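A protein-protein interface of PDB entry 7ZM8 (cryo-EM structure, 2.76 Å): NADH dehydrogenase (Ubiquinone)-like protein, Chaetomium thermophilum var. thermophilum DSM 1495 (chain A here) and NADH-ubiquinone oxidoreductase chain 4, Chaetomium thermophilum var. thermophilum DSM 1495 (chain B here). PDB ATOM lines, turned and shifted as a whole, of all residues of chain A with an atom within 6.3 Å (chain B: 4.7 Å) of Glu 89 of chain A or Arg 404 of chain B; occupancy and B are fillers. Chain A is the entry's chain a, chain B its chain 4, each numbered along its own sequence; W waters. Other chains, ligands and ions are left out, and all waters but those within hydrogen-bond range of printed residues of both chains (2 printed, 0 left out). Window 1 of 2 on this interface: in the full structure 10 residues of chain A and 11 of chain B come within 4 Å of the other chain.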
ATOM      1  N   ARG A  75     -21.770  27.738   8.488  1.00  0.00           N
ATOM      2  CA  ARG A  75     -23.045  27.096   8.760  1.00  0.00           C
ATOM      3  C   ARG A  75     -23.520  27.304  10.187  1.00  0.00           C
ATOM      4  O   ARG A  75     -24.625  26.871  10.517  1.00  0.00           O
ATOM      5  CB  ARG A  75     -22.957  25.608   8.424  1.00  0.00           C
ATOM      6  CG  ARG A  75     -23.273  25.337   6.970  1.00  0.00           C
ATOM      7  CD  ARG A  75     -23.063  23.902   6.582  1.00  0.00           C
ATOM      8  NE  ARG A  75     -21.759  23.717   5.960  1.00  0.00           N
ATOM      9  CZ  ARG A  75     -20.905  22.755   6.285  1.00  0.00           C
ATOM     10  NH1 ARG A  75     -19.737  22.673   5.671  1.00  0.00           N
ATOM     11  NH2 ARG A  75     -21.223  21.872   7.220  1.00  0.00           N
ATOM     12  N   ARG A  78     -26.724  29.207  10.079  1.00  0.00           N
ATOM     13  CA  ARG A  78     -27.939  28.560   9.627  1.00  0.00           C
ATOM     14  C   ARG A  78     -28.862  28.304  10.808  1.00  0.00           C
ATOM     15  O   ARG A  78     -28.467  28.385  11.972  1.00  0.00           O
ATOM     16  CB  ARG A  78     -27.621  27.253   8.907  1.00  0.00           C
ATOM     17  CG  ARG A  78     -26.787  27.427   7.666  1.00  0.00           C
ATOM     18  CD  ARG A  78     -26.852  26.200   6.804  1.00  0.00           C
ATOM     19  NE  ARG A  78     -26.144  26.403   5.551  1.00  0.00           N
ATOM     20  CZ  ARG A  78     -26.169  25.552   4.533  1.00  0.00           C
ATOM     21  NH1 ARG A  78     -25.492  25.824   3.432  1.00  0.00           N
ATOM     22  NH2 ARG A  78     -26.872  24.437   4.615  1.00  0.00           N
ATOM     23  N   TRP A  84     -33.085  19.874   8.682  1.00  0.00           N
ATOM     24  CA  TRP A  84     -31.820  19.466   8.094  1.00  0.00           C
ATOM     25  C   TRP A  84     -31.735  17.952   8.012  1.00  0.00           C
ATOM     26  O   TRP A  84     -32.076  17.242   8.958  1.00  0.00           O
ATOM     27  CB  TRP A  84     -30.648  20.000   8.912  1.00  0.00           C
ATOM     28  CG  TRP A  84     -30.618  21.476   9.059  1.00  0.00           C
ATOM     29  CD1 TRP A  84     -30.642  22.178  10.221  1.00  0.00           C
ATOM     30  CD2 TRP A  84     -30.551  22.443   8.007  1.00  0.00           C
ATOM     31  NE1 TRP A  84     -30.588  23.521   9.964  1.00  0.00           N
ATOM     32  CE2 TRP A  84     -30.534  23.711   8.610  1.00  0.00           C
ATOM     33  CE3 TRP A  84     -30.501  22.358   6.615  1.00  0.00           C
ATOM     34  CZ2 TRP A  84     -30.472  24.885   7.870  1.00  0.00           C
ATOM     35  CZ3 TRP A  84     -30.436  23.520   5.887  1.00  0.00           C
ATOM     36  CH2 TRP A  84     -30.422  24.769   6.515  1.00  0.00           C
ATOM     37  N   ASP A  86     -28.707  16.324   7.826  1.00  0.00           N
ATOM     38  CA  ASP A  86     -27.673  16.218   8.888  1.00  0.00           C
ATOM     39  C   ASP A  86     -27.881  17.402   9.823  1.00  0.00           C
ATOM     40  O   ASP A  86     -27.398  18.473   9.498  1.00  0.00           O
ATOM     41  CB  ASP A  86     -26.262  16.299   8.312  1.00  0.00           C
ATOM     42  CG  ASP A  86     -25.196  15.732   9.227  1.00  0.00           C
ATOM     43  OD1 ASP A  86     -25.508  15.465  10.402  1.00  0.00           O
ATOM     44  OD2 ASP A  86     -24.062  15.549   8.752  1.00  0.00           O
ATOM     45  N   LYS A  87     -28.577  17.193  10.930  1.00  0.00           N
ATOM     46  CA  LYS A  87     -28.887  18.281  11.881  1.00  0.00           C
ATOM     47  C   LYS A  87     -27.612  18.788  12.525  1.00  0.00           C
ATOM     48  O   LYS A  87     -27.552  19.986  12.811  1.00  0.00           O
ATOM     49  CB  LYS A  87     -29.850  17.785  12.957  1.00  0.00           C
ATOM     50  CG  LYS A  87     -31.202  17.299  12.456  1.00  0.00           C
ATOM     51  CD  LYS A  87     -32.195  18.415  12.217  1.00  0.00           C
ATOM     52  CE  LYS A  87     -33.588  17.897  11.932  1.00  0.00           C
ATOM     53  NZ  LYS A  87     -34.598  18.980  11.967  1.00  0.00           N
ATOM     54  N   GLN A  88     -26.668  17.902  12.806  1.00  0.00           N
ATOM     55  CA  GLN A  88     -25.439  18.292  13.525  1.00  0.00           C
ATOM     56  C   GLN A  88     -24.681  19.291  12.669  1.00  0.00           C
ATOM     57  O   GLN A  88     -24.150  20.261  13.218  1.00  0.00           O
ATOM     58  CB  GLN A  88     -24.555  17.076  13.768  1.00  0.00           C
ATOM     59  CG  GLN A  88     -25.215  16.004  14.614  1.00  0.00           C
ATOM     60  CD  GLN A  88     -24.311  14.807  14.761  1.00  0.00           C
ATOM     61  OE1 GLN A  88     -24.767  13.677  14.894  1.00  0.00           O
ATOM     62  NE2 GLN A  88     -23.015  15.051  14.714  1.00  0.00           N
ATOM     63  N   GLU A  89     -24.640  19.048  11.370  1.00  0.00           N
ATOM     64  CA  GLU A  89     -23.854  19.933  10.494  1.00  0.00           C
ATOM     65  C   GLU A  89     -24.750  21.020   9.920  1.00  0.00           C
ATOM     66  O   GLU A  89     -24.181  21.968   9.367  1.00  0.00           O
ATOM     67  CB  GLU A  89     -23.128  19.100   9.447  1.00  0.00           C
ATOM     68  CG  GLU A  89     -21.967  18.311  10.020  1.00  0.00           C
ATOM     69  CD  GLU A  89     -21.224  17.438   9.024  1.00  0.00           C
ATOM     70  OE1 GLU A  89     -21.659  17.374   7.856  1.00  0.00           O
ATOM     71  OE2 GLU A  89     -20.212  16.822   9.418  1.00  0.00           O
ATOM     72  N   ARG A  90     -26.071  20.909  10.081  1.00  0.00           N
ATOM     73  CA  ARG A  90     -27.032  21.875   9.479  1.00  0.00           C
ATOM     74  C   ARG A  90     -26.923  21.854   7.955  1.00  0.00           C
ATOM     75  O   ARG A  90     -26.747  22.911   7.354  1.00  0.00           O
ATOM     76  CB  ARG A  90     -26.922  23.251  10.136  1.00  0.00           C
ATOM     77  CG  ARG A  90     -27.003  23.213  11.652  1.00  0.00           C
ATOM     78  CD  ARG A  90     -26.853  24.601  12.220  1.00  0.00           C
ATOM     79  NE  ARG A  90     -26.679  24.548  13.657  1.00  0.00           N
ATOM     80  CZ  ARG A  90     -26.342  25.592  14.395  1.00  0.00           C
ATOM     81  NH1 ARG A  90     -26.141  26.764  13.822  1.00  0.00           N
ATOM     82  NH2 ARG A  90     -26.200  25.458  15.701  1.00  0.00           N
ATOM     83  N   ARG A  91     -27.041  20.666   7.367  1.00  0.00           N
ATOM     84  CA  ARG A  91     -26.892  20.509   5.901  1.00  0.00           C
ATOM     85  C   ARG A  91     -27.972  19.584   5.328  1.00  0.00           C
ATOM     86  O   ARG A  91     -28.588  18.879   6.115  1.00  0.00           O
ATOM     87  CB  ARG A  91     -25.458  20.006   5.672  1.00  0.00           C
ATOM     88  CG  ARG A  91     -25.001  19.922   4.225  1.00  0.00           C
ATOM     89  CD  ARG A  91     -23.747  19.099   4.024  1.00  0.00           C
ATOM     90  NE  ARG A  91     -23.483  19.084   2.598  1.00  0.00           N
ATOM     91  CZ  ARG A  91     -23.899  18.141   1.767  1.00  0.00           C
ATOM     92  NH1 ARG A  91     -24.568  17.100   2.228  1.00  0.00           N
ATOM     93  NH2 ARG A  91     -23.626  18.229   0.479  1.00  0.00           N
ATOM     94  N   HIS A 101     -15.568  24.153   1.905  1.00  0.00           N
ATOM     95  CA  HIS A 101     -16.411  23.336   2.820  1.00  0.00           C
ATOM     96  C   HIS A 101     -15.701  22.992   4.136  1.00  0.00           C
ATOM     97  O   HIS A 101     -16.389  23.001   5.171  1.00  0.00           O
ATOM     98  CB  HIS A 101     -16.898  22.103   2.039  1.00  0.00           C
ATOM     99  CG  HIS A 101     -17.993  21.319   2.677  1.00  0.00           C
ATOM    100  ND1 HIS A 101     -19.311  21.714   2.624  1.00  0.00           N
ATOM    101  CD2 HIS A 101     -17.980  20.145   3.341  1.00  0.00           C
ATOM    102  CE1 HIS A 101     -20.061  20.826   3.241  1.00  0.00           C
ATOM    103  NE2 HIS A 101     -19.268  19.857   3.692  1.00  0.00           N
ATOM    104  N   GLY A 105     -17.898  24.560   8.147  1.00  0.00           N
ATOM    105  CA  GLY A 105     -18.838  23.709   8.839  1.00  0.00           C
ATOM    106  C   GLY A 105     -18.888  23.960  10.330  1.00  0.00           C
ATOM    107  O   GLY A 105     -18.240  24.853  10.869  1.00  0.00           O
ATOM    108  N   MET A 106     -19.695  23.140  11.005  1.00  0.00           N
ATOM    109  CA  MET A 106     -19.876  23.289  12.442  1.00  0.00           C
ATOM    110  C   MET A 106     -18.609  22.947  13.208  1.00  0.00           C
ATOM    111  O   MET A 106     -18.408  23.440  14.321  1.00  0.00           O
ATOM    112  CB  MET A 106     -21.040  22.418  12.912  1.00  0.00           C
ATOM    113  CG  MET A 106     -22.407  22.949  12.496  1.00  0.00           C
ATOM    114  SD  MET A 106     -22.852  24.573  13.142  1.00  0.00           S
ATOM    115  CE  MET A 106     -22.247  24.484  14.821  1.00  0.00           C
ATOM    116  N   PHE A 107     -17.745  22.111  12.637  1.00  0.00           N
ATOM    117  CA  PHE A 107     -16.458  21.785  13.242  1.00  0.00           C
ATOM    118  C   PHE A 107     -15.389  22.623  12.551  1.00  0.00           C
ATOM    119  O   PHE A 107     -14.618  22.146  11.724  1.00  0.00           O
ATOM    120  CB  PHE A 107     -16.176  20.294  13.143  1.00  0.00           C
ATOM    121  CG  PHE A 107     -15.039  19.835  13.998  1.00  0.00           C
ATOM    122  CD1 PHE A 107     -14.514  20.660  14.982  1.00  0.00           C
ATOM    123  CD2 PHE A 107     -14.514  18.569  13.848  1.00  0.00           C
ATOM    124  CE1 PHE A 107     -13.480  20.240  15.771  1.00  0.00           C
ATOM    125  CE2 PHE A 107     -13.483  18.144  14.639  1.00  0.00           C
ATOM    126  CZ  PHE A 107     -12.965  18.980  15.604  1.00  0.00           C
ATOM    127  N   PHE B 402     -16.908  12.643   4.195  1.00  0.00           N
ATOM    128  CA  PHE B 402     -17.842  11.551   4.422  1.00  0.00           C
ATOM    129  C   PHE B 402     -17.637  10.840   5.749  1.00  0.00           C
ATOM    130  O   PHE B 402     -18.482  10.025   6.129  1.00  0.00           O
ATOM    131  CB  PHE B 402     -17.733  10.531   3.289  1.00  0.00           C
ATOM    132  CG  PHE B 402     -18.163  11.054   1.955  1.00  0.00           C
ATOM    133  CD1 PHE B 402     -19.493  11.322   1.699  1.00  0.00           C
ATOM    134  CD2 PHE B 402     -17.239  11.263   0.949  1.00  0.00           C
ATOM    135  CE1 PHE B 402     -19.893  11.791   0.472  1.00  0.00           C
ATOM    136  CE2 PHE B 402     -17.636  11.733  -0.282  1.00  0.00           C
ATOM    137  CZ  PHE B 402     -18.967  12.000  -0.519  1.00  0.00           C
ATOM    138  N   PHE B 403     -16.562  11.154   6.461  1.00  0.00           N
ATOM    139  CA  PHE B 403     -16.238  10.394   7.689  1.00  0.00           C
ATOM    140  C   PHE B 403     -16.542  11.223   8.930  1.00  0.00           C
ATOM    141  O   PHE B 403     -16.229  12.410   8.914  1.00  0.00           O
ATOM    142  CB  PHE B 403     -14.770   9.981   7.652  1.00  0.00           C
ATOM    143  CG  PHE B 403     -14.406   8.998   6.571  1.00  0.00           C
ATOM    144  CD1 PHE B 403     -14.559   7.638   6.769  1.00  0.00           C
ATOM    145  CD2 PHE B 403     -13.892   9.435   5.364  1.00  0.00           C
ATOM    146  CE1 PHE B 403     -14.221   6.739   5.775  1.00  0.00           C
ATOM    147  CE2 PHE B 403     -13.557   8.536   4.368  1.00  0.00           C
ATOM    148  CZ  PHE B 403     -13.720   7.189   4.577  1.00  0.00           C
ATOM    149  N   ARG B 404     -17.193  10.626   9.926  1.00  0.00           N
ATOM    150  CA  ARG B 404     -17.426  11.324  11.209  1.00  0.00           C
ATOM    151  C   ARG B 404     -17.786  10.293  12.275  1.00  0.00           C
ATOM    152  O   ARG B 404     -18.417   9.296  11.914  1.00  0.00           O
ATOM    153  CB  ARG B 404     -18.542  12.357  11.046  1.00  0.00           C
ATOM    154  CG  ARG B 404     -18.813  13.238  12.250  1.00  0.00           C
ATOM    155  CD  ARG B 404     -20.018  14.089  11.917  1.00  0.00           C
ATOM    156  NE  ARG B 404     -21.209  13.284  11.704  1.00  0.00           N
ATOM    157  CZ  ARG B 404     -22.381  13.768  11.318  1.00  0.00           C
ATOM    158  NH1 ARG B 404     -22.513  15.058  11.088  1.00  0.00           N
ATOM    159  NH2 ARG B 404     -23.414  12.964  11.156  1.00  0.00           N
ATOM    160  N   GLY B 405     -17.356  10.496  13.515  1.00  0.00           N
ATOM    161  CA  GLY B 405     -17.798   9.647  14.629  1.00  0.00           C
ATOM    162  C   GLY B 405     -17.459   8.197  14.471  1.00  0.00           C
ATOM    163  O   GLY B 405     -18.221   7.384  14.978  1.00  0.00           O
ATOM    164  N   LEU B 406     -16.342   7.877  13.830  1.00  0.00           N
ATOM    165  CA  LEU B 406     -16.063   6.473  13.576  1.00  0.00           C
ATOM    166  C   LEU B 406     -15.713   5.703  14.835  1.00  0.00           C
ATOM    167  O   LEU B 406     -15.776   4.472  14.819  1.00  0.00           O
ATOM    168  CB  LEU B 406     -14.929   6.334  12.569  1.00  0.00           C
ATOM    169  CG  LEU B 406     -15.356   6.283  11.110  1.00  0.00           C
ATOM    170  CD1 LEU B 406     -14.167   5.955  10.263  1.00  0.00           C
ATOM    171  CD2 LEU B 406     -16.451   5.254  10.913  1.00  0.00           C
ATOM    172  N   ARG B 471     -11.818  14.663  13.174  1.00  0.00           N
ATOM    173  CA  ARG B 471     -12.811  14.730  12.114  1.00  0.00           C
ATOM    174  C   ARG B 471     -13.255  13.353  11.648  1.00  0.00           C
ATOM    175  O   ARG B 471     -14.310  13.231  11.021  1.00  0.00           O
ATOM    176  CB  ARG B 471     -12.266  15.538  10.943  1.00  0.00           C
ATOM    177  CG  ARG B 471     -12.602  17.009  11.024  1.00  0.00           C
ATOM    178  CD  ARG B 471     -12.034  17.747   9.849  1.00  0.00           C
ATOM    179  NE  ARG B 471     -10.590  17.587   9.757  1.00  0.00           N
ATOM    180  CZ  ARG B 471      -9.880  17.909   8.686  1.00  0.00           C
ATOM    181  NH1 ARG B 471      -8.572  17.735   8.681  1.00  0.00           N
ATOM    182  NH2 ARG B 471     -10.486  18.396   7.617  1.00  0.00           N
ATOM    183  N   ILE B 472     -12.488  12.311  11.949  1.00  0.00           N
ATOM    184  CA  ILE B 472     -12.823  10.966  11.503  1.00  0.00           C
ATOM    185  C   ILE B 472     -13.308  10.135  12.684  1.00  0.00           C
ATOM    186  O   ILE B 472     -14.410   9.583  12.652  1.00  0.00           O
ATOM    187  CB  ILE B 472     -11.622  10.307  10.803  1.00  0.00           C
ATOM    188  CG1 ILE B 472     -11.227  11.120   9.569  1.00  0.00           C
ATOM    189  CG2 ILE B 472     -11.940   8.878  10.419  1.00  0.00           C
ATOM    190  CD1 ILE B 472      -9.901  10.760   8.999  1.00  0.00           C
ATOM    191  N   PHE B 474     -13.808  11.232  15.894  1.00  0.00           N
ATOM    192  CA  PHE B 474     -14.655  12.075  16.715  1.00  0.00           C
ATOM    193  C   PHE B 474     -15.390  13.023  15.782  1.00  0.00           C
ATOM    194  O   PHE B 474     -15.437  12.817  14.566  1.00  0.00           O
ATOM    195  CB  PHE B 474     -13.830  12.850  17.749  1.00  0.00           C
ATOM    196  CG  PHE B 474     -13.196  12.004  18.814  1.00  0.00           C
ATOM    197  CD1 PHE B 474     -13.549  10.680  18.988  1.00  0.00           C
ATOM    198  CD2 PHE B 474     -12.242  12.547  19.653  1.00  0.00           C
ATOM    199  CE1 PHE B 474     -12.956   9.915  19.966  1.00  0.00           C
ATOM    200  CE2 PHE B 474     -11.652  11.784  20.638  1.00  0.00           C
ATOM    201  CZ  PHE B 474     -12.012  10.467  20.792  1.00  0.00           C
ATOM    202  N   GLY B 475     -15.866  14.140  16.299  1.00  0.00           N
ATOM    203  CA  GLY B 475     -16.428  15.163  15.397  1.00  0.00           C
ATOM    204  C   GLY B 475     -17.919  15.092  15.303  1.00  0.00           C
ATOM    205  O   GLY B 475     -18.495  15.776  14.459  1.00  0.00           O
ATOM    206  N   GLY B 476     -18.520  14.297  16.172  1.00  0.00           N
ATOM    207  CA  GLY B 476     -19.964  14.119  16.102  1.00  0.00           C
ATOM    208  C   GLY B 476     -20.292  12.663  16.121  1.00  0.00           C
ATOM    209  O   GLY B 476     -19.414  11.878  16.444  1.00  0.00           O
ATOM    210  N   SER B 477     -21.528  12.328  15.812  1.00  0.00           N
ATOM    211  CA  SER B 477     -21.979  10.928  15.783  1.00  0.00           C
ATOM    212  C   SER B 477     -21.601  10.295  14.455  1.00  0.00           C
ATOM    213  O   SER B 477     -21.257  11.022  13.537  1.00  0.00           O
ATOM    214  CB  SER B 477     -23.442  10.870  16.035  1.00  0.00           C
ATOM    215  OG  SER B 477     -23.770  11.639  17.171  1.00  0.00           O
ATOM    216  N   VAL B 478     -21.703   8.979  14.375  1.00  0.00           N
ATOM    217  CA  VAL B 478     -21.399   8.249  13.117  1.00  0.00           C
ATOM    218  C   VAL B 478     -22.074   9.021  11.979  1.00  0.00           C
ATOM    219  O   VAL B 478     -23.244   9.393  12.130  1.00  0.00           O
ATOM    220  CB  VAL B 478     -21.827   6.767  13.205  1.00  0.00           C
ATOM    221  CG1 VAL B 478     -21.519   6.007  11.928  1.00  0.00           C
ATOM    222  CG2 VAL B 478     -21.222   6.063  14.402  1.00  0.00           C
ATOM    223  N   SER B 479     -21.357   9.203  10.864  1.00  0.00           N
ATOM    224  CA  SER B 479     -21.871  10.007   9.733  1.00  0.00           C
ATOM    225  C   SER B 479     -23.221   9.486   9.261  1.00  0.00           C
ATOM    226  O   SER B 479     -23.540   8.321   9.527  1.00  0.00           O
ATOM    227  CB  SER B 479     -20.884   9.959   8.619  1.00  0.00           C
ATOM    228  OG  SER B 479     -20.989   8.747   7.904  1.00  0.00           O
ATOM    229  N   LEU B 480     -23.937  10.292   8.488  1.00  0.00           N
ATOM    230  CA  LEU B 480     -25.232   9.856   7.932  1.00  0.00           C
ATOM    231  C   LEU B 480     -25.016   9.416   6.489  1.00  0.00           C
ATOM    232  O   LEU B 480     -25.962   8.901   5.886  1.00  0.00           O
ATOM    233  CB  LEU B 480     -26.234  11.007   8.049  1.00  0.00           C
ATOM    234  CG  LEU B 480     -26.583  11.446   9.466  1.00  0.00           C
ATOM    235  CD1 LEU B 480     -27.643  12.527   9.422  1.00  0.00           C
ATOM    236  CD2 LEU B 480     -27.068  10.267  10.289  1.00  0.00           C
ATOM    237  N   TYR B 481     -23.790   9.529   6.000  1.00  0.00           N
ATOM    238  CA  TYR B 481     -23.487   9.125   4.609  1.00  0.00           C
ATOM    239  C   TYR B 481     -23.271   7.615   4.582  1.00  0.00           C
ATOM    240  O   TYR B 481     -23.233   7.044   3.503  1.00  0.00           O
ATOM    241  CB  TYR B 481     -22.279   9.899   4.084  1.00  0.00           C
ATOM    242  CG  TYR B 481     -22.409  11.397   4.034  1.00  0.00           C
ATOM    243  CD1 TYR B 481     -23.107  12.022   3.018  1.00  0.00           C
ATOM    244  CD2 TYR B 481     -21.796  12.194   4.983  1.00  0.00           C
ATOM    245  CE1 TYR B 481     -23.221  13.400   2.963  1.00  0.00           C
ATOM    246  CE2 TYR B 481     -21.897  13.573   4.942  1.00  0.00           C
ATOM    247  CZ  TYR B 481     -22.618  14.177   3.932  1.00  0.00           C
ATOM    248  OH  TYR B 481     -22.719  15.534   3.891  1.00  0.00           O
HETATM  249  O   HOH W   1     -25.086  11.328  12.913  1.00  0.00           O
HETATM  250  O   HOH W   2     -23.101  12.978   7.843  1.00  0.00           O
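OD2 of Asp 86 of chain A is in salt-bridge range of NH1 of Arg 404 of chain B, 2.8 Å away. The side-chain amide oxygen (OE1) of Gln 88 of chain A is in hydrogen-bond range of the side-chain hydroxyl (OG) of Ser 477 of chain B, 3.2 Å away. The guanidinium group (NH1) of Arg 404 of chain B lies within salt-bridge range of the side-chain carboxylate (OE2) of Glu 89 of chain A (3.3 Å). OH of Tyr 481 of chain B is in hydrogen-bond range of NH1 of Arg 91 of chain A.
O of Arg 91 of chain A is in hydrogen-bond range of N of Asp 86 of chain A (3.1 Å). NE of Arg 404 of chain B lies within hydrogen-bond range of O of Ser 477 of chain B (2.9 Å). O of Arg 404 of chain B lies within hydrogen-bond range of N of Ser 479 of chain B, at 3.1 Å. The side-chain hydroxyl (OG) of Ser 479 of chain B lies close to the backbone NH (N) of Tyr 481 of chain B (3.5 Å).
CA of Asp 86 of chain A touches CD1 of Leu 480 of chain B (3.7 Å). NH1 of Arg 404 of chain B touches NE2 of Gln 88 of chain A, at 3.7 Å. Gly 476 of chain B touches Gln 88 of chain A. CD2 of Phe 107 of chain A touches CG of Arg 471 of chain B, at 3.8 Å.
Printed residues of chain B within 4 Å of Gln 88 of chain A: Arg 404 (3.7 Å), Gly 476 (3.5 Å) and Ser 477 (3.2 Å). Of chain B, only Arg 404 (3.3 Å) comes within 4 Å of Glu 89 of chain A. Of the printed residues of chain B, Arg 91 of chain A touches Tyr 481 (2.9 Å). Arg 404 of chain B touches just these residues of chain A: Asp 86, Gln 88 and Glu 89. Of the printed residues of chain A, Arg 471 of chain B touches Phe 107 (3.8 Å). Of the printed residues of chain A, Leu 480 of chain B touches Asp 86. Printed residues of chain A within 4 Å of Tyr 481 of chain B: Arg 91 (2.9 Å).
Of the 15 printed residues of chain B, 6 touch a printed residue of chain A. Printed residues of chain B that touch a printed residue of chain A: Arg 404, Arg 471, Gly 476, Ser 477, Leu 480 and Tyr 481. Hydrophobic or aromatic side chains of chain B within 4 Å of the printed part of chain A: Leu 480 and Tyr 481. Printed residues of chain A that touch a printed residue of chain B: Asp 86, Gln 88, Glu 89, Arg 91 and Phe 107. Hydrophobic or aromatic side chains of chain A that line the printed part of chain B: Phe 107. Along chain A the printed residues that touch a printed residue of chain B span positions 86 to 107.
Water W1 lies within hydrogen-bond range of O of Val 478 of chain B (2.8 Å), NH2 of Arg 404 of chain B (2.9 Å) and OE1 of Gln 88 of chain A (3.1 Å). Water W2 lies within hydrogen-bond range of N of Leu 480 of chain B (2.9 Å), OD2 of Asp 86 of chain A (2.9 Å) and NH2 of Arg 404 of chain B (3.3 Å).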
